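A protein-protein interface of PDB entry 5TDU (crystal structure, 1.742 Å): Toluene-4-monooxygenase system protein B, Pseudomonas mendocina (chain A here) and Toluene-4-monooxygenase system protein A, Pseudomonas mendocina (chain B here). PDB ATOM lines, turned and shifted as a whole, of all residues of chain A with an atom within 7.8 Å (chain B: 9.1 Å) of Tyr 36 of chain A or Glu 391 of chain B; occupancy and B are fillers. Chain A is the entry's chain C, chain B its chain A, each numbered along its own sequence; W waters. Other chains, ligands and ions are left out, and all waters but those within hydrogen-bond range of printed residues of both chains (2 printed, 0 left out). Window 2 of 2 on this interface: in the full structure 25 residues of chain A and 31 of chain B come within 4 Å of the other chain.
Trp 338 of chain B touches Gln 17 of chain A.
Thr 392 of chain B touches Gln 17 of chain A (CG2 to NE2, 3.7 Å).
Leu 393 of chain B touches Gln 17 of chain A.
Phe 454 of chain B touches Leu 18 of chain A.
His 37 of chain A touches Thr 392 of chain B.
Asn 40 of chain A touches Leu 387 of chain B (O to CD1, 3.3 Å).
Arg 41 of chain A touches Leu 387 of chain B (NH1 to CA, 3.6 Å).
NH2 of Arg 42 of chain A touches CE2 of Tyr 337 of chain B, 3.3 Å away.
O of Leu 18 of chain A sits at hydrogen-bond distance from OG1 of Thr 392 of chain B (2.5 Å).
The side-chain carboxylate (OE1) of Glu 391 of chain B is in hydrogen-bond range of the side-chain hydroxyl (OH) of Tyr 36 of chain A (2.8 Å).
The backbone carbonyl oxygen of Ser 389 of chain B is in hydrogen-bond range of the guanidinium group of Arg 41 of chain A.
N of Leu 18 of chain A is in hydrogen-bond range of O of Leu 393 of chain B, at 2.9 Å.
OH of Tyr 337 of chain B lies within hydrogen-bond range of NH1 of Arg 41 of chain A, 2.9 Å away.
The guanidinium group (NH1) of Arg 41 of chain A lies within hydrogen-bond range of the backbone carbonyl oxygen (O) of Asp 386 of chain B (3.3 Å).
OE2 of Glu 391 of chain B is in salt-bridge range of NH2 of Arg 41 of chain A, 3.1 Å away.
The side-chain hydroxyl (OH) of Tyr 337 of chain B is in hydrogen-bond range of the backbone carbonyl oxygen (O) of Leu 387 of chain B.
NE1 of Trp 338 of chain B lies within hydrogen-bond range of O of Thr 392 of chain B (2.8 Å).
The backbone carbonyl oxygen (O) of Tyr 36 of chain A lies within hydrogen-bond range of the guanidinium group (NE) of Arg 41 of chain A (3.2 Å).
The side-chain amide nitrogen (NE2) of Gln 17 of chain A lies close to the guanidinium group (NH1) of Arg 42 of chain A (3.3 Å).
O of His 37 of chain A lies close to OE1 of Gln 17 of chain A, 3.4 Å away.
Water W2 lies within hydrogen-bond range of N of Glu 391 of chain B (2.9 Å) and ND1 of His 37 of chain A (3.0 Å).
Water W1 lies within hydrogen-bond range of the backbone carbonyl oxygen (O) of Leu 387 of chain B (2.9 Å) and the backbone carbonyl oxygen (O) of Arg 41 of chain A (2.9 Å).
Of the 18 printed residues of chain A, 7 touch a printed residue of chain B.
Hydrophobic or aromatic side chains of chain A within 4 Å of the printed part of chain B: Leu 18, Tyr 36 and His 37.
Hydrophobic or aromatic side chains of chain B within 4 Å of the printed part of chain A: Tyr 337, Trp 338, Leu 387 and Phe 454.
Among the printed residues, 15 pairs touch across the chains.
Among the printed residues, Asp or Glu carboxylates within 4 Å of a Lys or Arg side-chain nitrogen of the other chain: Arg 41 of chain A with Glu 391 of chain B (3.1 Å).
Printed residues of chain A within 4 Å of Glu 391 of chain B: Tyr 36 (2.8 Å) and Arg 41 (3.1 Å).
No residue of chain B comes within 4 Å of Ala 35 of chain A.
Of the printed residues of chain A, Leu 393 of chain B touches Gln 17 (3.8 Å) and Leu 18 (2.9 Å).
Printed residues of chain B within 4 Å of Arg 41 of chain A: Tyr 337, Asp 386, Leu 387, Ser 389 and Glu 391.
Of the printed residues of chain B, Leu 18 of chain A touches Thr 392, Leu 393 and Phe 454.
Val 30 of chain A touches none of the printed residues of chain B.
Met 50 of chain A touches none of the printed residues of chain B.
The nearest residue of chain B that does not touch Tyr 36 of chain A is Leu 387 of chain B (6.2 Å).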
ATOM      1  N   PHE A  10      -8.595  11.189 -16.262  1.00  0.00           N
ATOM      2  CA  PHE A  10      -8.008   9.925 -16.688  1.00  0.00           C
ATOM      3  C   PHE A  10      -8.458   8.769 -15.796  1.00  0.00           C
ATOM      4  O   PHE A  10      -8.539   8.910 -14.573  1.00  0.00           O
ATOM      5  CB  PHE A  10      -6.481  10.016 -16.688  1.00  0.00           C
ATOM      6  CG  PHE A  10      -5.815   8.928 -17.479  1.00  0.00           C
ATOM      7  CD1 PHE A  10      -5.651   7.658 -16.941  1.00  0.00           C
ATOM      8  CD2 PHE A  10      -5.360   9.177 -18.760  1.00  0.00           C
ATOM      9  CE1 PHE A  10      -5.034   6.651 -17.673  1.00  0.00           C
ATOM     10  CE2 PHE A  10      -4.750   8.180 -19.498  1.00  0.00           C
ATOM     11  CZ  PHE A  10      -4.588   6.915 -18.954  1.00  0.00           C
ATOM     12  N   GLN A  17      -7.869  17.470 -14.809  1.00  0.00           N
ATOM     13  CA  GLN A  17      -6.780  18.408 -15.044  1.00  0.00           C
ATOM     14  C   GLN A  17      -6.988  19.218 -16.301  1.00  0.00           C
ATOM     15  O   GLN A  17      -7.622  18.759 -17.257  1.00  0.00           O
ATOM     16  CB  GLN A  17      -5.434  17.679 -15.158  1.00  0.00           C
ATOM     17  CG  GLN A  17      -4.909  17.069 -13.879  1.00  0.00           C
ATOM     18  CD  GLN A  17      -3.666  16.233 -14.124  1.00  0.00           C
ATOM     19  OE1 GLN A  17      -3.680  15.308 -14.945  1.00  0.00           O
ATOM     20  NE2 GLN A  17      -2.585  16.560 -13.431  1.00  0.00           N
ATOM     21  N   LEU A  18      -6.412  20.412 -16.315  1.00  0.00           N
ATOM     22  CA  LEU A  18      -6.309  21.177 -17.548  1.00  0.00           C
ATOM     23  C   LEU A  18      -5.242  20.565 -18.469  1.00  0.00           C
ATOM     24  O   LEU A  18      -4.074  20.466 -18.099  1.00  0.00           O
ATOM     25  CB  LEU A  18      -5.975  22.632 -17.237  1.00  0.00           C
ATOM     26  CG  LEU A  18      -5.624  23.495 -18.450  1.00  0.00           C
ATOM     27  CD1 LEU A  18      -6.858  23.740 -19.304  1.00  0.00           C
ATOM     28  CD2 LEU A  18      -4.998  24.807 -18.001  1.00  0.00           C
ATOM     29  N   VAL A  19      -5.659  20.128 -19.653  1.00  0.00           N
ATOM     30  CA  VAL A  19      -4.720  19.655 -20.674  1.00  0.00           C
ATOM     31  C   VAL A  19      -4.996  20.422 -21.947  1.00  0.00           C
ATOM     32  O   VAL A  19      -6.119  20.424 -22.438  1.00  0.00           O
ATOM     33  CB  VAL A  19      -4.838  18.144 -20.919  1.00  0.00           C
ATOM     34  CG1 VAL A  19      -3.832  17.698 -21.985  1.00  0.00           C
ATOM     35  CG2 VAL A  19      -4.625  17.375 -19.622  1.00  0.00           C
ATOM     36  N   VAL A  30      -4.807  13.112 -28.426  1.00  0.00           N
ATOM     37  CA  VAL A  30      -5.392  13.707 -27.234  1.00  0.00           C
ATOM     38  C   VAL A  30      -5.157  12.792 -26.042  1.00  0.00           C
ATOM     39  O   VAL A  30      -4.756  13.250 -24.972  1.00  0.00           O
ATOM     40  CB  VAL A  30      -6.892  13.977 -27.419  1.00  0.00           C
ATOM     41  CG1 VAL A  30      -7.533  14.404 -26.076  1.00  0.00           C
ATOM     42  CG2 VAL A  30      -7.119  15.030 -28.497  1.00  0.00           C
ATOM     43  N   ALA A  31      -5.422  11.502 -26.219  1.00  0.00           N
ATOM     44  CA  ALA A  31      -5.313  10.554 -25.112  1.00  0.00           C
ATOM     45  C   ALA A  31      -3.885  10.499 -24.583  1.00  0.00           C
ATOM     46  O   ALA A  31      -3.661  10.410 -23.374  1.00  0.00           O
ATOM     47  CB  ALA A  31      -5.771   9.173 -25.545  1.00  0.00           C
ATOM     48  N   GLU A  32      -2.924  10.551 -25.502  1.00  0.00           N
ATOM     49  CA  GLU A  32      -1.512  10.560 -25.144  1.00  0.00           C
ATOM     50  C   GLU A  32      -1.141  11.788 -24.308  1.00  0.00           C
ATOM     51  O   GLU A  32      -0.481  11.668 -23.276  1.00  0.00           O
ATOM     52  CB  GLU A  32      -0.646  10.509 -26.407  1.00  0.00           C
ATOM     53  CG  GLU A  32       0.654   9.789 -26.195  1.00  0.00           C
ATOM     54  CD  GLU A  32       0.442   8.357 -25.756  1.00  0.00           C
ATOM     55  OE1 GLU A  32      -0.384   7.656 -26.385  1.00  0.00           O
ATOM     56  OE2 GLU A  32       1.091   7.937 -24.774  1.00  0.00           O
ATOM     57  N   LYS A  33      -1.566  12.965 -24.760  1.00  0.00           N
ATOM     58  CA  LYS A  33      -1.227  14.210 -24.084  1.00  0.00           C
ATOM     59  C   LYS A  33      -1.792  14.249 -22.659  1.00  0.00           C
ATOM     60  O   LYS A  33      -1.161  14.786 -21.747  1.00  0.00           O
ATOM     61  CB  LYS A  33      -1.730  15.413 -24.889  1.00  0.00           C
ATOM     62  CG  LYS A  33      -0.956  15.656 -26.171  1.00  0.00           C
ATOM     63  CD  LYS A  33      -1.380  16.945 -26.865  1.00  0.00           C
ATOM     64  CE  LYS A  33      -0.482  17.237 -28.063  1.00  0.00           C
ATOM     65  NZ  LYS A  33      -0.900  18.455 -28.813  1.00  0.00           N
ATOM     66  N   VAL A  34      -2.975  13.677 -22.470  1.00  0.00           N
ATOM     67  CA  VAL A  34      -3.562  13.590 -21.140  1.00  0.00           C
ATOM     68  C   VAL A  34      -2.792  12.571 -20.304  1.00  0.00           C
ATOM     69  O   VAL A  34      -2.429  12.842 -19.160  1.00  0.00           O
ATOM     70  CB  VAL A  34      -5.057  13.230 -21.205  1.00  0.00           C
ATOM     71  CG1 VAL A  34      -5.618  13.034 -19.805  1.00  0.00           C
ATOM     72  CG2 VAL A  34      -5.826  14.310 -21.951  1.00  0.00           C
ATOM     73  N   ALA A  35      -2.532  11.403 -20.888  1.00  0.00           N
ATOM     74  CA  ALA A  35      -1.840  10.335 -20.172  1.00  0.00           C
ATOM     75  C   ALA A  35      -0.508  10.835 -19.619  1.00  0.00           C
ATOM     76  O   ALA A  35      -0.091  10.439 -18.520  1.00  0.00           O
ATOM     77  CB  ALA A  35      -1.623   9.126 -21.084  1.00  0.00           C
ATOM     78  N   TYR A  36       0.140  11.728 -20.368  1.00  0.00           N
ATOM     79  CA  TYR A  36       1.432  12.247 -19.958  1.00  0.00           C
ATOM     80  C   TYR A  36       1.370  12.726 -18.519  1.00  0.00           C
ATOM     81  O   TYR A  36       2.312  12.536 -17.749  1.00  0.00           O
ATOM     82  CB  TYR A  36       1.901  13.399 -20.853  1.00  0.00           C
ATOM     83  CG  TYR A  36       3.191  14.003 -20.342  1.00  0.00           C
ATOM     84  CD1 TYR A  36       4.429  13.517 -20.765  1.00  0.00           C
ATOM     85  CD2 TYR A  36       3.175  15.034 -19.403  1.00  0.00           C
ATOM     86  CE1 TYR A  36       5.614  14.056 -20.278  1.00  0.00           C
ATOM     87  CE2 TYR A  36       4.353  15.574 -18.912  1.00  0.00           C
ATOM     88  CZ  TYR A  36       5.566  15.083 -19.350  1.00  0.00           C
ATOM     89  OH  TYR A  36       6.729  15.631 -18.855  1.00  0.00           O
ATOM     90  N   HIS A  37       0.253  13.351 -18.168  1.00  0.00           N
ATOM     91  CA  HIS A  37       0.114  13.974 -16.865  1.00  0.00           C
ATOM     92  C   HIS A  37      -0.474  13.031 -15.816  1.00  0.00           C
ATOM     93  O   HIS A  37      -0.812  13.472 -14.716  1.00  0.00           O
ATOM     94  CB  HIS A  37      -0.762  15.222 -16.968  1.00  0.00           C
ATOM     95  CG  HIS A  37      -0.208  16.286 -17.863  1.00  0.00           C
ATOM     96  ND1 HIS A  37       0.858  17.081 -17.504  1.00  0.00           N
ATOM     97  CD2 HIS A  37      -0.591  16.707 -19.093  1.00  0.00           C
ATOM     98  CE1 HIS A  37       1.113  17.941 -18.474  1.00  0.00           C
ATOM     99  NE2 HIS A  37       0.249  17.733 -19.451  1.00  0.00           N
ATOM    100  N   CYS A  38      -0.581  11.744 -16.140  1.00  0.00           N
ATOM    101  CA  CYS A  38      -1.315  10.807 -15.292  1.00  0.00           C
ATOM    102  C   CYS A  38      -0.610   9.472 -15.078  1.00  0.00           C
ATOM    103  O   CYS A  38      -0.341   9.077 -13.935  1.00  0.00           O
ATOM    104  CB  CYS A  38      -2.704  10.550 -15.881  1.00  0.00           C
ATOM    105  SG  CYS A  38      -3.700  12.041 -16.061  1.00  0.00           S
ATOM    106  N   VAL A  39      -0.347   8.767 -16.176  1.00  0.00           N
ATOM    107  CA  VAL A  39       0.302   7.466 -16.122  1.00  0.00           C
ATOM    108  C   VAL A  39       1.729   7.638 -15.614  1.00  0.00           C
ATOM    109  O   VAL A  39       2.458   8.538 -16.052  1.00  0.00           O
ATOM    110  CB  VAL A  39       0.279   6.768 -17.507  1.00  0.00           C
ATOM    111  CG1 VAL A  39       0.947   5.395 -17.437  1.00  0.00           C
ATOM    112  CG2 VAL A  39      -1.147   6.640 -18.005  1.00  0.00           C
ATOM    113  N   ASN A  40       2.113   6.778 -14.676  1.00  0.00           N
ATOM    114  CA  ASN A  40       3.427   6.846 -14.049  1.00  0.00           C
ATOM    115  C   ASN A  40       3.561   8.034 -13.109  1.00  0.00           C
ATOM    116  O   ASN A  40       4.657   8.341 -12.649  1.00  0.00           O
ATOM    117  CB  ASN A  40       4.524   6.892 -15.112  1.00  0.00           C
ATOM    118  CG  ASN A  40       4.736   5.556 -15.769  1.00  0.00           C
ATOM    119  OD1 ASN A  40       4.559   4.515 -15.136  1.00  0.00           O
ATOM    120  ND2 ASN A  40       5.109   5.569 -17.044  1.00  0.00           N
ATOM    121  N   ARG A  41       2.443   8.704 -12.831  1.00  0.00           N
ATOM    122  CA  ARG A  41       2.411   9.733 -11.794  1.00  0.00           C
ATOM    123  C   ARG A  41       1.505   9.296 -10.668  1.00  0.00           C
ATOM    124  O   ARG A  41       1.917   9.229  -9.509  1.00  0.00           O
ATOM    125  CB  ARG A  41       1.933  11.070 -12.353  1.00  0.00           C
ATOM    126  CG  ARG A  41       2.904  11.652 -13.356  1.00  0.00           C
ATOM    127  CD  ARG A  41       2.421  12.970 -13.911  1.00  0.00           C
ATOM    128  NE  ARG A  41       3.370  13.463 -14.899  1.00  0.00           N
ATOM    129  CZ  ARG A  41       4.433  14.198 -14.604  1.00  0.00           C
ATOM    130  NH1 ARG A  41       4.667  14.555 -13.347  1.00  0.00           N
ATOM    131  NH2 ARG A  41       5.258  14.583 -15.568  1.00  0.00           N
ATOM    132  N   ARG A  42       0.259   9.006 -11.022  1.00  0.00           N
ATOM    133  CA  ARG A  42      -0.720   8.555 -10.048  1.00  0.00           C
ATOM    134  C   ARG A  42      -1.470   7.331 -10.560  1.00  0.00           C
ATOM    135  O   ARG A  42      -2.254   6.727  -9.833  1.00  0.00           O
ATOM    136  CB  ARG A  42      -1.695   9.688  -9.712  1.00  0.00           C
ATOM    137  CG  ARG A  42      -1.039  10.888  -9.036  1.00  0.00           C
ATOM    138  CD  ARG A  42      -2.002  12.066  -8.943  1.00  0.00           C
ATOM    139  NE  ARG A  42      -2.552  12.398 -10.253  1.00  0.00           N
ATOM    140  CZ  ARG A  42      -1.972  13.208 -11.135  1.00  0.00           C
ATOM    141  NH1 ARG A  42      -2.553  13.439 -12.305  1.00  0.00           N
ATOM    142  NH2 ARG A  42      -0.816  13.787 -10.852  1.00  0.00           N
ATOM    143  N   MET A  50      -6.177   3.490 -25.334  1.00  0.00           N
ATOM    144  CA  MET A  50      -6.810   4.634 -24.692  1.00  0.00           C
ATOM    145  C   MET A  50      -7.828   5.249 -25.644  1.00  0.00           C
ATOM    146  O   MET A  50      -7.548   5.422 -26.831  1.00  0.00           O
ATOM    147  CB  MET A  50      -5.767   5.669 -24.278  1.00  0.00           C
ATOM    148  CG  MET A  50      -4.877   5.226 -23.131  1.00  0.00           C
ATOM    149  SD  MET A  50      -3.699   6.509 -22.663  1.00  0.00           S
ATOM    150  CE  MET A  50      -2.726   6.647 -24.167  1.00  0.00           C
ATOM    151  N   TYR B 337       0.368  16.799  -4.192  1.00  0.00           N
ATOM    152  CA  TYR B 337       1.006  16.696  -5.509  1.00  0.00           C
ATOM    153  C   TYR B 337       1.330  18.099  -6.026  1.00  0.00           C
ATOM    154  O   TYR B 337       2.377  18.312  -6.629  1.00  0.00           O
ATOM    155  CB  TYR B 337       0.133  15.935  -6.508  1.00  0.00           C
ATOM    156  CG  TYR B 337       0.936  15.398  -7.680  1.00  0.00           C
ATOM    157  CD1 TYR B 337       1.611  14.183  -7.587  1.00  0.00           C
ATOM    158  CD2 TYR B 337       1.040  16.119  -8.862  1.00  0.00           C
ATOM    159  CE1 TYR B 337       2.354  13.688  -8.659  1.00  0.00           C
ATOM    160  CE2 TYR B 337       1.790  15.631  -9.938  1.00  0.00           C
ATOM    161  CZ  TYR B 337       2.440  14.421  -9.821  1.00  0.00           C
ATOM    162  OH  TYR B 337       3.180  13.939 -10.882  1.00  0.00           O
ATOM    163  N   TRP B 338       0.449  19.062  -5.752  1.00  0.00           N
ATOM    164  CA  TRP B 338       0.686  20.452  -6.144  1.00  0.00           C
ATOM    165  C   TRP B 338       1.219  21.250  -4.956  1.00  0.00           C
ATOM    166  O   TRP B 338       0.979  22.455  -4.843  1.00  0.00           O
ATOM    167  CB  TRP B 338      -0.593  21.101  -6.710  1.00  0.00           C
ATOM    168  CG  TRP B 338      -0.803  20.811  -8.187  1.00  0.00           C
ATOM    169  CD1 TRP B 338      -0.470  21.620  -9.236  1.00  0.00           C
ATOM    170  CD2 TRP B 338      -1.385  19.636  -8.753  1.00  0.00           C
ATOM    171  NE1 TRP B 338      -0.791  21.008 -10.424  1.00  0.00           N
ATOM    172  CE2 TRP B 338      -1.360  19.791 -10.157  1.00  0.00           C
ATOM    173  CE3 TRP B 338      -1.917  18.461  -8.212  1.00  0.00           C
ATOM    174  CZ2 TRP B 338      -1.862  18.820 -11.029  1.00  0.00           C
ATOM    175  CZ3 TRP B 338      -2.409  17.497  -9.072  1.00  0.00           C
ATOM    176  CH2 TRP B 338      -2.368  17.678 -10.474  1.00  0.00           C
ATOM    177  N   THR B 340       3.826  22.631  -4.313  1.00  0.00           N
ATOM    178  CA  THR B 340       4.625  23.820  -4.592  1.00  0.00           C
ATOM    179  C   THR B 340       3.758  25.081  -4.682  1.00  0.00           C
ATOM    180  O   THR B 340       4.278  26.197  -4.651  1.00  0.00           O
ATOM    181  CB  THR B 340       5.458  23.654  -5.891  1.00  0.00           C
ATOM    182  OG1 THR B 340       6.251  24.829  -6.098  1.00  0.00           O
ATOM    183  CG2 THR B 340       4.557  23.417  -7.097  1.00  0.00           C
ATOM    184  N   MET B 385      11.968  11.835  -9.370  1.00  0.00           N
ATOM    185  CA  MET B 385      11.283  12.945  -8.711  1.00  0.00           C
ATOM    186  C   MET B 385      10.532  13.837  -9.686  1.00  0.00           C
ATOM    187  O   MET B 385       9.651  14.599  -9.285  1.00  0.00           O
ATOM    188  CB  MET B 385      12.281  13.782  -7.906  1.00  0.00           C
ATOM    189  CG  MET B 385      13.055  12.978  -6.880  1.00  0.00           C
ATOM    190  SD  MET B 385      12.004  11.976  -5.805  1.00  0.00           S
ATOM    191  CE  MET B 385      11.067  13.250  -4.966  1.00  0.00           C
ATOM    192  N   ASP B 386      10.870  13.732 -10.968  1.00  0.00           N
ATOM    193  CA  ASP B 386      10.169  14.499 -11.988  1.00  0.00           C
ATOM    194  C   ASP B 386       8.707  14.056 -12.110  1.00  0.00           C
ATOM    195  O   ASP B 386       7.857  14.829 -12.545  1.00  0.00           O
ATOM    196  CB  ASP B 386      10.869  14.354 -13.337  1.00  0.00           C
ATOM    197  CG  ASP B 386      10.989  12.915 -13.765  1.00  0.00           C
ATOM    198  OD1 ASP B 386      10.470  12.581 -14.845  1.00  0.00           O
ATOM    199  OD2 ASP B 386      11.593  12.117 -13.014  1.00  0.00           O
ATOM    200  N   LEU B 387       8.424  12.812 -11.730  1.00  0.00           N
ATOM    201  CA  LEU B 387       7.068  12.268 -11.827  1.00  0.00           C
ATOM    202  C   LEU B 387       6.263  12.555 -10.557  1.00  0.00           C
ATOM    203  O   LEU B 387       5.087  12.187 -10.459  1.00  0.00           O
ATOM    204  CB  LEU B 387       7.100  10.759 -12.087  1.00  0.00           C
ATOM    205  CG  LEU B 387       7.929  10.315 -13.304  1.00  0.00           C
ATOM    206  CD1 LEU B 387       7.863   8.805 -13.477  1.00  0.00           C
ATOM    207  CD2 LEU B 387       7.469  11.031 -14.567  1.00  0.00           C
ATOM    208  N   VAL B 388       6.905  13.201  -9.586  1.00  0.00           N
ATOM    209  CA  VAL B 388       6.239  13.550  -8.331  1.00  0.00           C
ATOM    210  C   VAL B 388       5.983  15.049  -8.274  1.00  0.00           C
ATOM    211  O   VAL B 388       5.605  15.595  -7.230  1.00  0.00           O
ATOM    212  CB  VAL B 388       7.054  13.098  -7.111  1.00  0.00           C
ATOM    213  CG1 VAL B 388       7.632  11.716  -7.343  1.00  0.00           C
ATOM    214  CG2 VAL B 388       8.155  14.103  -6.804  1.00  0.00           C
ATOM    215  N   SER B 389       6.178  15.722  -9.402  1.00  0.00           N
ATOM    216  CA  SER B 389       5.878  17.146  -9.497  1.00  0.00           C
ATOM    217  C   SER B 389       5.099  17.414 -10.778  1.00  0.00           C
ATOM    218  O   SER B 389       5.468  16.932 -11.850  1.00  0.00           O
ATOM    219  CB  SER B 389       7.150  17.987  -9.453  1.00  0.00           C
ATOM    220  OG  SER B 389       7.672  18.045  -8.137  1.00  0.00           O
ATOM    221  N   PRO B 390       4.012  18.188 -10.670  1.00  0.00           N
ATOM    222  CA  PRO B 390       3.089  18.405 -11.785  1.00  0.00           C
ATOM    223  C   PRO B 390       3.602  19.399 -12.816  1.00  0.00           C
ATOM    224  O   PRO B 390       4.385  20.292 -12.488  1.00  0.00           O
ATOM    225  CB  PRO B 390       1.848  18.964 -11.089  1.00  0.00           C
ATOM    226  CG  PRO B 390       2.427  19.773  -9.979  1.00  0.00           C
ATOM    227  CD  PRO B 390       3.633  18.989  -9.490  1.00  0.00           C
ATOM    228  N   GLU B 391       3.140  19.253 -14.051  1.00  0.00           N
ATOM    229  CA  GLU B 391       3.505  20.187 -15.103  1.00  0.00           C
ATOM    230  C   GLU B 391       2.283  20.829 -15.747  1.00  0.00           C
ATOM    231  O   GLU B 391       2.379  21.440 -16.812  1.00  0.00           O
ATOM    232  CB  GLU B 391       4.354  19.475 -16.160  1.00  0.00           C
ATOM    233  CG  GLU B 391       5.602  18.815 -15.580  1.00  0.00           C
ATOM    234  CD  GLU B 391       6.325  17.942 -16.586  1.00  0.00           C
ATOM    235  OE1 GLU B 391       6.124  18.142 -17.804  1.00  0.00           O
ATOM    236  OE2 GLU B 391       7.096  17.054 -16.159  1.00  0.00           O
ATOM    237  N   THR B 392       1.128  20.683 -15.107  1.00  0.00           N
ATOM    238  CA  THR B 392      -0.068  21.391 -15.540  1.00  0.00           C
ATOM    239  C   THR B 392      -0.867  21.821 -14.315  1.00  0.00           C
ATOM    240  O   THR B 392      -0.444  21.580 -13.182  1.00  0.00           O
ATOM    241  CB  THR B 392      -0.951  20.530 -16.467  1.00  0.00           C
ATOM    242  OG1 THR B 392      -2.012  21.334 -16.996  1.00  0.00           O
ATOM    243  CG2 THR B 392      -1.532  19.336 -15.719  1.00  0.00           C
ATOM    244  N   LEU B 393      -2.007  22.467 -14.550  1.00  0.00           N
ATOM    245  CA  LEU B 393      -2.886  22.897 -13.462  1.00  0.00           C
ATOM    246  C   LEU B 393      -4.071  21.963 -13.322  1.00  0.00           C
ATOM    247  O   LEU B 393      -4.570  21.425 -14.314  1.00  0.00           O
ATOM    248  CB  LEU B 393      -3.396  24.321 -13.691  1.00  0.00           C
ATOM    249  CG  LEU B 393      -2.411  25.480 -13.576  1.00  0.00           C
ATOM    250  CD1 LEU B 393      -3.149  26.806 -13.674  1.00  0.00           C
ATOM    251  CD2 LEU B 393      -1.634  25.382 -12.276  1.00  0.00           C
ATOM    252  N   PRO B 394      -4.535  21.766 -12.083  1.00  0.00           N
ATOM    253  CA  PRO B 394      -5.780  21.030 -11.875  1.00  0.00           C
ATOM    254  C   PRO B 394      -6.966  21.860 -12.357  1.00  0.00           C
ATOM    255  O   PRO B 394      -6.887  23.091 -12.354  1.00  0.00           O
ATOM    256  CB  PRO B 394      -5.827  20.832 -10.351  1.00  0.00           C
ATOM    257  CG  PRO B 394      -5.000  21.950  -9.803  1.00  0.00           C
ATOM    258  CD  PRO B 394      -3.922  22.211 -10.815  1.00  0.00           C
ATOM    259  N   PHE B 454      -6.211  31.973 -15.836  1.00  0.00           N
ATOM    260  CA  PHE B 454      -5.068  31.396 -16.544  1.00  0.00           C
ATOM    261  C   PHE B 454      -5.385  31.268 -18.039  1.00  0.00           C
ATOM    262  O   PHE B 454      -4.543  31.530 -18.899  1.00  0.00           O
ATOM    263  CB  PHE B 454      -4.734  30.032 -15.928  1.00  0.00           C
ATOM    264  CG  PHE B 454      -3.434  29.430 -16.394  1.00  0.00           C
ATOM    265  CD1 PHE B 454      -2.220  29.927 -15.944  1.00  0.00           C
ATOM    266  CD2 PHE B 454      -3.431  28.335 -17.235  1.00  0.00           C
ATOM    267  CE1 PHE B 454      -1.028  29.363 -16.345  1.00  0.00           C
ATOM    268  CE2 PHE B 454      -2.240  27.765 -17.652  1.00  0.00           C
ATOM    269  CZ  PHE B 454      -1.034  28.279 -17.205  1.00  0.00           C
ATOM    270  N   MET B 462       1.899  32.319 -19.126  1.00  0.00           N
ATOM    271  CA  MET B 462       0.913  31.267 -18.935  1.00  0.00           C
ATOM    272  C   MET B 462       1.610  29.922 -18.749  1.00  0.00           C
ATOM    273  O   MET B 462       1.558  29.042 -19.620  1.00  0.00           O
ATOM    274  CB  MET B 462      -0.045  31.219 -20.119  1.00  0.00           C
ATOM    275  CG  MET B 462      -1.360  30.530 -19.816  1.00  0.00           C
ATOM    276  SD  MET B 462      -2.361  30.367 -21.293  1.00  0.00           S
ATOM    277  CE  MET B 462      -1.390  29.168 -22.191  1.00  0.00           C
ATOM    278  N   THR B 463       2.281  29.798 -17.608  1.00  0.00           N
ATOM    279  CA  THR B 463       3.049  28.617 -17.234  1.00  0.00           C
ATOM    280  C   THR B 463       2.833  28.365 -15.746  1.00  0.00           C
ATOM    281  O   THR B 463       2.321  29.235 -15.053  1.00  0.00           O
ATOM    282  CB  THR B 463       4.550  28.810 -17.494  1.00  0.00           C
ATOM    283  OG1 THR B 463       5.028  29.881 -16.669  1.00  0.00           O
ATOM    284  CG2 THR B 463       4.814  29.145 -18.965  1.00  0.00           C
ATOM    285  N   LEU B 464       3.232  27.198 -15.249  1.00  0.00           N
ATOM    286  CA  LEU B 464       3.125  26.926 -13.818  1.00  0.00           C
ATOM    287  C   LEU B 464       3.939  27.950 -13.027  1.00  0.00           C
ATOM    288  O   LEU B 464       3.496  28.438 -11.989  1.00  0.00           O
ATOM    289  CB  LEU B 464       3.591  25.506 -13.487  1.00  0.00           C
ATOM    290  CG  LEU B 464       3.643  25.170 -11.992  1.00  0.00           C
ATOM    291  CD1 LEU B 464       2.239  25.077 -11.390  1.00  0.00           C
ATOM    292  CD2 LEU B 464       4.437  23.893 -11.729  1.00  0.00           C
ATOM    293  N   GLU B 465       5.130  28.285 -13.518  1.00  0.00           N
ATOM    294  CA  GLU B 465       5.954  29.269 -12.830  1.00  0.00           C
ATOM    295  C   GLU B 465       5.272  30.631 -12.846  1.00  0.00           C
ATOM    296  O   GLU B 465       5.291  31.350 -11.848  1.00  0.00           O
ATOM    297  CB  GLU B 465       7.361  29.370 -13.446  1.00  0.00           C
ATOM    298  CG  GLU B 465       8.207  30.447 -12.761  1.00  0.00           C
ATOM    299  CD  GLU B 465       9.681  30.434 -13.148  1.00  0.00           C
ATOM    300  OE1 GLU B 465      10.356  31.457 -12.906  1.00  0.00           O
ATOM    301  OE2 GLU B 465      10.169  29.412 -13.676  1.00  0.00           O
HETATM  302  O   HOH W   1       4.616   9.961  -8.664  1.00  0.00           O
HETATM  303  O   HOH W   2       1.864  16.781 -14.738  1.00  0.00           O
